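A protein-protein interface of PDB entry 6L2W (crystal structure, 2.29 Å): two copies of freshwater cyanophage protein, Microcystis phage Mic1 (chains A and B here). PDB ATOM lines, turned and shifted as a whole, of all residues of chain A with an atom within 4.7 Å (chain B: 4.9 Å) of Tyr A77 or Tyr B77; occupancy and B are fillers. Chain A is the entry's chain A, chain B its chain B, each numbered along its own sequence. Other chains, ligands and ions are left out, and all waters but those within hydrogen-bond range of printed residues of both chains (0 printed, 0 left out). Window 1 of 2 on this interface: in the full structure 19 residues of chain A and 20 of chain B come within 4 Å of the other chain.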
ATOM      1  N   HIS A   9      19.646 -25.256 -29.279  1.00  0.00           N
ATOM      2  CA  HIS A   9      20.147 -26.590 -29.574  1.00  0.00           C
ATOM      3  C   HIS A   9      20.100 -27.387 -28.267  1.00  0.00           C
ATOM      4  O   HIS A   9      20.511 -26.898 -27.229  1.00  0.00           O
ATOM      5  CB  HIS A   9      21.539 -26.535 -30.228  1.00  0.00           C
ATOM      6  CG  HIS A   9      22.367 -25.369 -29.801  1.00  0.00           C
ATOM      7  ND1 HIS A   9      22.673 -25.130 -28.469  1.00  0.00           N
ATOM      8  CD2 HIS A   9      22.941 -24.373 -30.514  1.00  0.00           C
ATOM      9  CE1 HIS A   9      23.392 -24.027 -28.380  1.00  0.00           C
ATOM     10  NE2 HIS A   9      23.572 -23.543 -29.622  1.00  0.00           N
ATOM     11  N   PHE A  11      19.022 -31.611 -26.450  1.00  0.00           N
ATOM     12  CA  PHE A  11      18.729 -33.035 -26.612  1.00  0.00           C
ATOM     13  C   PHE A  11      17.513 -33.469 -25.778  1.00  0.00           C
ATOM     14  O   PHE A  11      16.741 -34.325 -26.224  1.00  0.00           O
ATOM     15  CB  PHE A  11      19.974 -33.857 -26.286  1.00  0.00           C
ATOM     16  CG  PHE A  11      20.884 -34.020 -27.467  1.00  0.00           C
ATOM     17  CD1 PHE A  11      20.731 -35.095 -28.326  1.00  0.00           C
ATOM     18  CD2 PHE A  11      21.861 -33.081 -27.741  1.00  0.00           C
ATOM     19  CE1 PHE A  11      21.573 -35.254 -29.414  1.00  0.00           C
ATOM     20  CE2 PHE A  11      22.700 -33.237 -28.833  1.00  0.00           C
ATOM     21  CZ  PHE A  11      22.549 -34.318 -29.675  1.00  0.00           C
ATOM     22  N   PHE A  18      17.638 -34.904 -30.584  1.00  0.00           N
ATOM     23  CA  PHE A  18      18.212 -33.578 -30.828  1.00  0.00           C
ATOM     24  C   PHE A  18      17.250 -32.666 -31.602  1.00  0.00           C
ATOM     25  O   PHE A  18      16.652 -33.058 -32.596  1.00  0.00           O
ATOM     26  CB  PHE A  18      19.513 -33.720 -31.621  1.00  0.00           C
ATOM     27  CG  PHE A  18      20.173 -32.419 -32.014  1.00  0.00           C
ATOM     28  CD1 PHE A  18      20.774 -31.606 -31.064  1.00  0.00           C
ATOM     29  CD2 PHE A  18      20.201 -32.014 -33.339  1.00  0.00           C
ATOM     30  CE1 PHE A  18      21.378 -30.414 -31.429  1.00  0.00           C
ATOM     31  CE2 PHE A  18      20.807 -30.825 -33.704  1.00  0.00           C
ATOM     32  CZ  PHE A  18      21.392 -30.026 -32.750  1.00  0.00           C
ATOM     33  N   GLY A  63      19.808 -17.040 -19.511  1.00  0.00           N
ATOM     34  CA  GLY A  63      21.018 -17.507 -18.844  1.00  0.00           C
ATOM     35  C   GLY A  63      22.254 -17.425 -19.744  1.00  0.00           C
ATOM     36  O   GLY A  63      23.266 -18.091 -19.459  1.00  0.00           O
ATOM     37  N   ILE A  64      22.208 -16.613 -20.814  1.00  0.00           N
ATOM     38  CA  ILE A  64      23.424 -16.314 -21.573  1.00  0.00           C
ATOM     39  C   ILE A  64      24.296 -15.338 -20.787  1.00  0.00           C
ATOM     40  O   ILE A  64      23.825 -14.287 -20.387  1.00  0.00           O
ATOM     41  CB  ILE A  64      23.102 -15.764 -22.971  1.00  0.00           C
ATOM     42  CG1 ILE A  64      22.434 -16.842 -23.825  1.00  0.00           C
ATOM     43  CG2 ILE A  64      24.366 -15.203 -23.622  1.00  0.00           C
ATOM     44  CD1 ILE A  64      21.886 -16.342 -25.125  1.00  0.00           C
ATOM     45  N   GLU A  65      25.571 -15.692 -20.606  1.00  0.00           N
ATOM     46  CA  GLU A  65      26.512 -14.874 -19.834  1.00  0.00           C
ATOM     47  C   GLU A  65      27.740 -14.543 -20.682  1.00  0.00           C
ATOM     48  O   GLU A  65      27.974 -15.135 -21.741  1.00  0.00           O
ATOM     49  CB  GLU A  65      26.976 -15.635 -18.595  1.00  0.00           C
ATOM     50  CG  GLU A  65      25.843 -16.076 -17.683  1.00  0.00           C
ATOM     51  CD  GLU A  65      26.219 -16.104 -16.213  1.00  0.00           C
ATOM     52  OE1 GLU A  65      27.387 -16.460 -15.904  1.00  0.00           O
ATOM     53  OE2 GLU A  65      25.356 -15.741 -15.388  1.00  0.00           O
ATOM     54  N   TYR A  75      30.783 -15.551 -29.867  1.00  0.00           N
ATOM     55  CA  TYR A  75      29.684 -16.383 -29.477  1.00  0.00           C
ATOM     56  C   TYR A  75      29.486 -16.286 -27.972  1.00  0.00           C
ATOM     57  O   TYR A  75      30.441 -16.056 -27.228  1.00  0.00           O
ATOM     58  CB  TYR A  75      29.967 -17.841 -29.832  1.00  0.00           C
ATOM     59  CG  TYR A  75      30.468 -18.027 -31.230  1.00  0.00           C
ATOM     60  CD1 TYR A  75      29.576 -18.165 -32.278  1.00  0.00           C
ATOM     61  CD2 TYR A  75      31.819 -17.964 -31.518  1.00  0.00           C
ATOM     62  CE1 TYR A  75      30.030 -18.349 -33.573  1.00  0.00           C
ATOM     63  CE2 TYR A  75      32.292 -18.117 -32.814  1.00  0.00           C
ATOM     64  CZ  TYR A  75      31.392 -18.337 -33.843  1.00  0.00           C
ATOM     65  OH  TYR A  75      31.823 -18.461 -35.131  1.00  0.00           O
ATOM     66  N   TRP A  76      28.237 -16.468 -27.560  1.00  0.00           N
ATOM     67  CA  TRP A  76      27.856 -16.473 -26.138  1.00  0.00           C
ATOM     68  C   TRP A  76      26.922 -17.654 -25.907  1.00  0.00           C
ATOM     69  O   TRP A  76      25.892 -17.705 -26.560  1.00  0.00           O
ATOM     70  CB  TRP A  76      27.151 -15.167 -25.755  1.00  0.00           C
ATOM     71  CG  TRP A  76      28.056 -13.991 -25.812  1.00  0.00           C
ATOM     72  CD1 TRP A  76      28.750 -13.436 -24.786  1.00  0.00           C
ATOM     73  CD2 TRP A  76      28.394 -13.237 -26.987  1.00  0.00           C
ATOM     74  NE1 TRP A  76      29.527 -12.408 -25.246  1.00  0.00           N
ATOM     75  CE2 TRP A  76      29.314 -12.248 -26.589  1.00  0.00           C
ATOM     76  CE3 TRP A  76      28.023 -13.316 -28.330  1.00  0.00           C
ATOM     77  CZ2 TRP A  76      29.848 -11.328 -27.481  1.00  0.00           C
ATOM     78  CZ3 TRP A  76      28.559 -12.416 -29.211  1.00  0.00           C
ATOM     79  CH2 TRP A  76      29.455 -11.432 -28.792  1.00  0.00           C
ATOM     80  N   TYR A  77      27.246 -18.542 -24.982  1.00  0.00           N
ATOM     81  CA  TYR A  77      26.356 -19.660 -24.680  1.00  0.00           C
ATOM     82  C   TYR A  77      25.613 -19.431 -23.363  1.00  0.00           C
ATOM     83  O   TYR A  77      26.115 -18.739 -22.503  1.00  0.00           O
ATOM     84  CB  TYR A  77      27.144 -20.966 -24.637  1.00  0.00           C
ATOM     85  CG  TYR A  77      27.513 -21.499 -25.997  1.00  0.00           C
ATOM     86  CD1 TYR A  77      28.621 -21.021 -26.680  1.00  0.00           C
ATOM     87  CD2 TYR A  77      26.769 -22.508 -26.584  1.00  0.00           C
ATOM     88  CE1 TYR A  77      28.978 -21.537 -27.914  1.00  0.00           C
ATOM     89  CE2 TYR A  77      27.117 -23.042 -27.812  1.00  0.00           C
ATOM     90  CZ  TYR A  77      28.220 -22.547 -28.485  1.00  0.00           C
ATOM     91  OH  TYR A  77      28.543 -23.051 -29.712  1.00  0.00           O
ATOM     92  N   SER A  78      24.421 -20.026 -23.239  1.00  0.00           N
ATOM     93  CA  SER A  78      23.719 -20.158 -21.930  1.00  0.00           C
ATOM     94  C   SER A  78      24.429 -21.197 -21.056  1.00  0.00           C
ATOM     95  O   SER A  78      25.068 -22.104 -21.568  1.00  0.00           O
ATOM     96  CB  SER A  78      22.262 -20.510 -22.104  1.00  0.00           C
ATOM     97  OG  SER A  78      22.114 -21.746 -22.779  1.00  0.00           O
ATOM     98  N   GLY A  79      24.338 -21.046 -19.741  1.00  0.00           N
ATOM     99  CA  GLY A  79      24.917 -22.014 -18.792  1.00  0.00           C
ATOM    100  C   GLY A  79      24.534 -23.459 -19.101  1.00  0.00           C
ATOM    101  O   GLY A  79      25.404 -24.316 -19.164  1.00  0.00           O
ATOM    102  N   MET A  81      23.690 -24.569 -21.848  1.00  0.00           N
ATOM    103  CA  MET A  81      24.084 -24.776 -23.265  1.00  0.00           C
ATOM    104  C   MET A  81      22.873 -24.946 -24.191  1.00  0.00           C
ATOM    105  O   MET A  81      23.062 -25.469 -25.257  1.00  0.00           O
ATOM    106  CB  MET A  81      25.048 -25.955 -23.409  1.00  0.00           C
ATOM    107  CG  MET A  81      26.341 -25.766 -22.645  1.00  0.00           C
ATOM    108  SD  MET A  81      27.552 -24.682 -23.364  1.00  0.00           S
ATOM    109  CE  MET A  81      27.295 -25.069 -25.076  1.00  0.00           C
ATOM    110  N   TYR A  83      21.112 -22.450 -25.556  1.00  0.00           N
ATOM    111  CA  TYR A  83      21.084 -21.351 -26.474  1.00  0.00           C
ATOM    112  C   TYR A  83      22.506 -20.832 -26.698  1.00  0.00           C
ATOM    113  O   TYR A  83      23.385 -21.013 -25.871  1.00  0.00           O
ATOM    114  CB  TYR A  83      20.237 -20.206 -25.912  1.00  0.00           C
ATOM    115  CG  TYR A  83      18.827 -20.550 -25.517  1.00  0.00           C
ATOM    116  CD1 TYR A  83      18.529 -20.974 -24.235  1.00  0.00           C
ATOM    117  CD2 TYR A  83      17.784 -20.423 -26.419  1.00  0.00           C
ATOM    118  CE1 TYR A  83      17.233 -21.290 -23.859  1.00  0.00           C
ATOM    119  CE2 TYR A  83      16.482 -20.740 -26.061  1.00  0.00           C
ATOM    120  CZ  TYR A  83      16.205 -21.168 -24.778  1.00  0.00           C
ATOM    121  OH  TYR A  83      14.924 -21.467 -24.438  1.00  0.00           O
ATOM    122  N   HIS A  84      22.694 -20.117 -27.802  1.00  0.00           N
ATOM    123  CA  HIS A  84      23.849 -19.279 -27.931  1.00  0.00           C
ATOM    124  C   HIS A  84      23.546 -18.100 -28.856  1.00  0.00           C
ATOM    125  O   HIS A  84      22.777 -18.233 -29.800  1.00  0.00           O
ATOM    126  CB  HIS A  84      25.047 -20.094 -28.413  1.00  0.00           C
ATOM    127  CG  HIS A  84      25.174 -20.225 -29.892  1.00  0.00           C
ATOM    128  ND1 HIS A  84      24.620 -21.270 -30.581  1.00  0.00           N
ATOM    129  CD2 HIS A  84      25.830 -19.475 -30.797  1.00  0.00           C
ATOM    130  CE1 HIS A  84      24.921 -21.169 -31.855  1.00  0.00           C
ATOM    131  NE2 HIS A  84      25.671 -20.072 -32.012  1.00  0.00           N
ATOM    132  N   HIS B   9      32.837 -26.718 -25.255  1.00  0.00           N
ATOM    133  CA  HIS B   9      32.261 -25.607 -24.515  1.00  0.00           C
ATOM    134  C   HIS B   9      31.459 -26.151 -23.347  1.00  0.00           C
ATOM    135  O   HIS B   9      30.697 -27.085 -23.489  1.00  0.00           O
ATOM    136  CB  HIS B   9      31.354 -24.755 -25.402  1.00  0.00           C
ATOM    137  CG  HIS B   9      30.672 -25.562 -26.452  1.00  0.00           C
ATOM    138  ND1 HIS B   9      29.897 -26.656 -26.141  1.00  0.00           N
ATOM    139  CD2 HIS B   9      30.658 -25.451 -27.797  1.00  0.00           C
ATOM    140  CE1 HIS B   9      29.461 -27.214 -27.263  1.00  0.00           C
ATOM    141  NE2 HIS B   9      29.898 -26.485 -28.286  1.00  0.00           N
ATOM    142  N   PHE B  18      33.038 -19.897 -18.209  1.00  0.00           N
ATOM    143  CA  PHE B  18      32.828 -20.462 -19.519  1.00  0.00           C
ATOM    144  C   PHE B  18      34.154 -21.047 -19.986  1.00  0.00           C
ATOM    145  O   PHE B  18      35.148 -20.338 -20.003  1.00  0.00           O
ATOM    146  CB  PHE B  18      32.354 -19.387 -20.505  1.00  0.00           C
ATOM    147  CG  PHE B  18      32.015 -19.916 -21.873  1.00  0.00           C
ATOM    148  CD1 PHE B  18      31.052 -20.900 -22.033  1.00  0.00           C
ATOM    149  CD2 PHE B  18      32.640 -19.419 -23.003  1.00  0.00           C
ATOM    150  CE1 PHE B  18      30.747 -21.402 -23.289  1.00  0.00           C
ATOM    151  CE2 PHE B  18      32.319 -19.907 -24.261  1.00  0.00           C
ATOM    152  CZ  PHE B  18      31.384 -20.906 -24.399  1.00  0.00           C
ATOM    153  N   GLY B  63      30.504 -38.693 -28.435  1.00  0.00           N
ATOM    154  CA  GLY B  63      29.037 -38.685 -28.275  1.00  0.00           C
ATOM    155  C   GLY B  63      28.351 -37.724 -29.240  1.00  0.00           C
ATOM    156  O   GLY B  63      27.222 -37.316 -29.038  1.00  0.00           O
ATOM    157  N   ILE B  64      29.019 -37.395 -30.323  1.00  0.00           N
ATOM    158  CA  ILE B  64      28.435 -36.542 -31.324  1.00  0.00           C
ATOM    159  C   ILE B  64      27.579 -37.414 -32.246  1.00  0.00           C
ATOM    160  O   ILE B  64      28.013 -38.462 -32.714  1.00  0.00           O
ATOM    161  CB  ILE B  64      29.530 -35.769 -32.078  1.00  0.00           C
ATOM    162  CG1 ILE B  64      30.126 -34.678 -31.186  1.00  0.00           C
ATOM    163  CG2 ILE B  64      29.005 -35.207 -33.389  1.00  0.00           C
ATOM    164  CD1 ILE B  64      31.410 -34.071 -31.724  1.00  0.00           C
ATOM    165  N   GLU B  65      26.375 -36.936 -32.500  1.00  0.00           N
ATOM    166  CA  GLU B  65      25.368 -37.719 -33.152  1.00  0.00           C
ATOM    167  C   GLU B  65      24.857 -36.978 -34.395  1.00  0.00           C
ATOM    168  O   GLU B  65      24.932 -35.757 -34.506  1.00  0.00           O
ATOM    169  CB  GLU B  65      24.195 -37.969 -32.201  1.00  0.00           C
ATOM    170  CG  GLU B  65      24.470 -38.936 -31.056  1.00  0.00           C
ATOM    171  CD  GLU B  65      23.350 -38.960 -30.021  1.00  0.00           C
ATOM    172  OE1 GLU B  65      22.181 -39.131 -30.416  1.00  0.00           O
ATOM    173  OE2 GLU B  65      23.635 -38.762 -28.825  1.00  0.00           O
ATOM    174  N   PHE B  73      22.013 -27.928 -42.588  1.00  0.00           N
ATOM    175  CA  PHE B  73      22.466 -27.617 -41.212  1.00  0.00           C
ATOM    176  C   PHE B  73      23.815 -28.314 -41.071  1.00  0.00           C
ATOM    177  O   PHE B  73      23.843 -29.518 -41.192  1.00  0.00           O
ATOM    178  CB  PHE B  73      21.411 -28.028 -40.189  1.00  0.00           C
ATOM    179  CG  PHE B  73      21.684 -27.620 -38.768  1.00  0.00           C
ATOM    180  CD1 PHE B  73      21.449 -26.331 -38.340  1.00  0.00           C
ATOM    181  CD2 PHE B  73      22.144 -28.535 -37.846  1.00  0.00           C
ATOM    182  CE1 PHE B  73      21.681 -25.962 -37.029  1.00  0.00           C
ATOM    183  CE2 PHE B  73      22.380 -28.163 -36.537  1.00  0.00           C
ATOM    184  CZ  PHE B  73      22.152 -26.879 -36.130  1.00  0.00           C
ATOM    185  N   TYR B  75      26.052 -28.532 -38.486  1.00  0.00           N
ATOM    186  CA  TYR B  75      26.531 -28.662 -37.124  1.00  0.00           C
ATOM    187  C   TYR B  75      26.033 -29.974 -36.527  1.00  0.00           C
ATOM    188  O   TYR B  75      24.906 -30.369 -36.738  1.00  0.00           O
ATOM    189  CB  TYR B  75      26.037 -27.503 -36.250  1.00  0.00           C
ATOM    190  CG  TYR B  75      26.297 -26.133 -36.823  1.00  0.00           C
ATOM    191  CD1 TYR B  75      25.395 -25.527 -37.674  1.00  0.00           C
ATOM    192  CD2 TYR B  75      27.470 -25.465 -36.558  1.00  0.00           C
ATOM    193  CE1 TYR B  75      25.633 -24.269 -38.209  1.00  0.00           C
ATOM    194  CE2 TYR B  75      27.725 -24.208 -37.080  1.00  0.00           C
ATOM    195  CZ  TYR B  75      26.801 -23.598 -37.905  1.00  0.00           C
ATOM    196  OH  TYR B  75      27.065 -22.361 -38.439  1.00  0.00           O
ATOM    197  N   TRP B  76      26.900 -30.583 -35.738  1.00  0.00           N
ATOM    198  CA  TRP B  76      26.593 -31.794 -35.005  1.00  0.00           C
ATOM    199  C   TRP B  76      27.035 -31.622 -33.555  1.00  0.00           C
ATOM    200  O   TRP B  76      28.207 -31.419 -33.303  1.00  0.00           O
ATOM    201  CB  TRP B  76      27.307 -32.999 -35.631  1.00  0.00           C
ATOM    202  CG  TRP B  76      26.894 -33.288 -37.040  1.00  0.00           C
ATOM    203  CD1 TRP B  76      25.999 -34.228 -37.472  1.00  0.00           C
ATOM    204  CD2 TRP B  76      27.354 -32.610 -38.219  1.00  0.00           C
ATOM    205  NE1 TRP B  76      25.867 -34.178 -38.839  1.00  0.00           N
ATOM    206  CE2 TRP B  76      26.696 -33.207 -39.327  1.00  0.00           C
ATOM    207  CE3 TRP B  76      28.246 -31.558 -38.444  1.00  0.00           C
ATOM    208  CZ2 TRP B  76      26.922 -32.803 -40.639  1.00  0.00           C
ATOM    209  CZ3 TRP B  76      28.459 -31.152 -39.746  1.00  0.00           C
ATOM    210  CH2 TRP B  76      27.797 -31.757 -40.824  1.00  0.00           C
ATOM    211  N   TYR B  77      26.104 -31.817 -32.635  1.00  0.00           N
ATOM    212  CA  TYR B  77      26.332 -31.646 -31.223  1.00  0.00           C
ATOM    213  C   TYR B  77      26.453 -32.998 -30.510  1.00  0.00           C
ATOM    214  O   TYR B  77      25.849 -33.989 -30.911  1.00  0.00           O
ATOM    215  CB  TYR B  77      25.202 -30.802 -30.630  1.00  0.00           C
ATOM    216  CG  TYR B  77      25.388 -29.328 -30.878  1.00  0.00           C
ATOM    217  CD1 TYR B  77      24.882 -28.717 -32.012  1.00  0.00           C
ATOM    218  CD2 TYR B  77      26.125 -28.557 -30.001  1.00  0.00           C
ATOM    219  CE1 TYR B  77      25.073 -27.367 -32.253  1.00  0.00           C
ATOM    220  CE2 TYR B  77      26.312 -27.200 -30.220  1.00  0.00           C
ATOM    221  CZ  TYR B  77      25.799 -26.608 -31.357  1.00  0.00           C
ATOM    222  OH  TYR B  77      26.000 -25.272 -31.559  1.00  0.00           O
ATOM    223  N   SER B  78      27.200 -32.998 -29.441  1.00  0.00           N
ATOM    224  CA  SER B  78      27.289 -34.204 -28.598  1.00  0.00           C
ATOM    225  C   SER B  78      26.042 -34.254 -27.716  1.00  0.00           C
ATOM    226  O   SER B  78      25.439 -33.215 -27.495  1.00  0.00           O
ATOM    227  CB  SER B  78      28.547 -34.219 -27.799  1.00  0.00           C
ATOM    228  OG  SER B  78      28.576 -33.173 -26.866  1.00  0.00           O
ATOM    229  N   GLY B  79      25.673 -35.409 -27.226  1.00  0.00           N
ATOM    230  CA  GLY B  79      24.478 -35.531 -26.378  1.00  0.00           C
ATOM    231  C   GLY B  79      24.579 -34.733 -25.096  1.00  0.00           C
ATOM    232  O   GLY B  79      23.563 -34.213 -24.684  1.00  0.00           O
ATOM    233  N   MET B  81      26.218 -31.963 -24.796  1.00  0.00           N
ATOM    234  CA  MET B  81      26.391 -30.582 -25.308  1.00  0.00           C
ATOM    235  C   MET B  81      27.781 -30.031 -24.995  1.00  0.00           C
ATOM    236  O   MET B  81      27.952 -28.857 -25.143  1.00  0.00           O
ATOM    237  CB  MET B  81      25.297 -29.629 -24.829  1.00  0.00           C
ATOM    238  CG  MET B  81      23.940 -29.982 -25.366  1.00  0.00           C
ATOM    239  SD  MET B  81      23.731 -29.735 -27.114  1.00  0.00           S
ATOM    240  CE  MET B  81      24.093 -28.000 -27.244  1.00  0.00           C
ATOM    241  N   TYR B  83      30.560 -30.712 -26.751  1.00  0.00           N
ATOM    242  CA  TYR B  83      31.352 -30.617 -27.986  1.00  0.00           C
ATOM    243  C   TYR B  83      30.419 -30.381 -29.167  1.00  0.00           C
ATOM    244  O   TYR B  83      29.284 -30.784 -29.158  1.00  0.00           O
ATOM    245  CB  TYR B  83      32.163 -31.889 -28.286  1.00  0.00           C
ATOM    246  CG  TYR B  83      32.872 -32.462 -27.095  1.00  0.00           C
ATOM    247  CD1 TYR B  83      34.051 -31.908 -26.642  1.00  0.00           C
ATOM    248  CD2 TYR B  83      32.324 -33.502 -26.377  1.00  0.00           C
ATOM    249  CE1 TYR B  83      34.685 -32.378 -25.512  1.00  0.00           C
ATOM    250  CE2 TYR B  83      32.940 -33.989 -25.237  1.00  0.00           C
ATOM    251  CZ  TYR B  83      34.111 -33.408 -24.793  1.00  0.00           C
ATOM    252  OH  TYR B  83      34.717 -33.843 -23.656  1.00  0.00           O
ATOM    253  N   HIS B  84      30.932 -29.793 -30.217  1.00  0.00           N
ATOM    254  CA  HIS B  84      30.224 -29.916 -31.464  1.00  0.00           C
ATOM    255  C   HIS B  84      31.202 -29.864 -32.627  1.00  0.00           C
ATOM    256  O   HIS B  84      32.333 -29.389 -32.485  1.00  0.00           O
ATOM    257  CB  HIS B  84      29.112 -28.870 -31.569  1.00  0.00           C
ATOM    258  CG  HIS B  84      29.569 -27.535 -32.029  1.00  0.00           C
ATOM    259  ND1 HIS B  84      30.175 -26.657 -31.182  1.00  0.00           N
ATOM    260  CD2 HIS B  84      29.483 -26.922 -33.234  1.00  0.00           C
ATOM    261  CE1 HIS B  84      30.430 -25.530 -31.841  1.00  0.00           C
ATOM    262  NE2 HIS B  84      30.025 -25.670 -33.106  1.00  0.00           N
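A ring nitrogen (NE2) of His A9 sits at hydrogen-bond distance from a ring nitrogen (ND1) of His A84 (2.7 Å). The backbone NH (N) of Met A81 sits at hydrogen-bond distance from the side-chain hydroxyl (OG) of Ser A78 (3.4 Å). NE2 of His B9 lies within hydrogen-bond range of ND1 of His B84 (2.9 Å). The backbone carbonyl oxygen (O) of Tyr B77 sits at hydrogen-bond distance from the backbone NH (N) of Glu B65. The backbone NH (N) of Met B81 lies within hydrogen-bond range of the side-chain hydroxyl (OG) of Ser B78. The backbone NH (N) of Ser B78 sits at hydrogen-bond distance from the backbone carbonyl oxygen (O) of Tyr B83, 3.1 Å away.
His A9 touches Met B81 (ND1 to CE, 3.4 Å). O of Ser B78 touches CE2 of Phe A11, 3.0 Å away. Phe A11 touches Gly B79. CD1 of Tyr B77 touches CZ of Phe A18, at 3.8 Å. OH of Tyr A77 touches CD2 of His B9, at 3.7 Å. CD1 of Tyr A77 touches CZ of Phe B18 (3.6 Å). OH of Tyr B77 touches OH of Tyr A77 (3.8 Å). OH of Tyr A77 touches CE1 of His B84, 3.8 Å away. CE of Met A81 touches ND1 of His B9, 3.2 Å away. CE of Met B81 touches O of Met A81, at 3.4 Å.
Tyr A77 touches just these residues of chain B: His B9, Phe B18, Tyr B77 and His B84. Of the printed residues of chain A, Tyr B77 touches His A9 (3.4 Å), Phe A11 (3.5 Å), Phe A18 (3.8 Å) and Tyr A77 (3.8 Å). Of the printed residues of chain A, His B9 touches Tyr A77 and Met A81. Printed residues of chain A within 4 Å of Ser B78: Phe A11 (3.0 Å). Of the printed residues of chain A, His B84 touches Tyr A77. Of the printed residues of chain B, Phe A18 touches Tyr B77 (3.8 Å). The nearest residue of chain A that does not touch Tyr B77 is His A84 (4.3 Å). The nearest printed residue of chain B that does not touch Phe A11 is Glu B65 (4.1 Å).
Printed residues of chain A that touch a printed residue of chain B: His A9, Phe A11, Phe A18, Tyr A77 and Met A81. Hydrophobic or aromatic side chains of chain A within 4 Å of the printed part of chain B: His A9, Phe A11, Phe A18, Tyr A77 and Met A81. Of the 14 printed residues of chain B, 7 touch a printed residue of chain A. Hydrophobic or aromatic side chains of chain B within 4 Å of the printed part of chain A: His B9, Phe B18, Tyr B77, Met B81 and His B84. Along chain B the printed residues that touch a printed residue of chain A span positions 9 to 84.
His A9 touches Tyr B77, and with the chains exchanged Tyr A77 touches His B9. Phe A18 touches Tyr B77, and with the chains exchanged Tyr A77 touches Phe B18. Tyr A77 touches its own counterpart, Tyr B77. Met A81 touches its own counterpart, Met B81. Of the 13 pairs that touch across the chains among the printed residues, 8 have their exchanged pair printed and touching as well.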
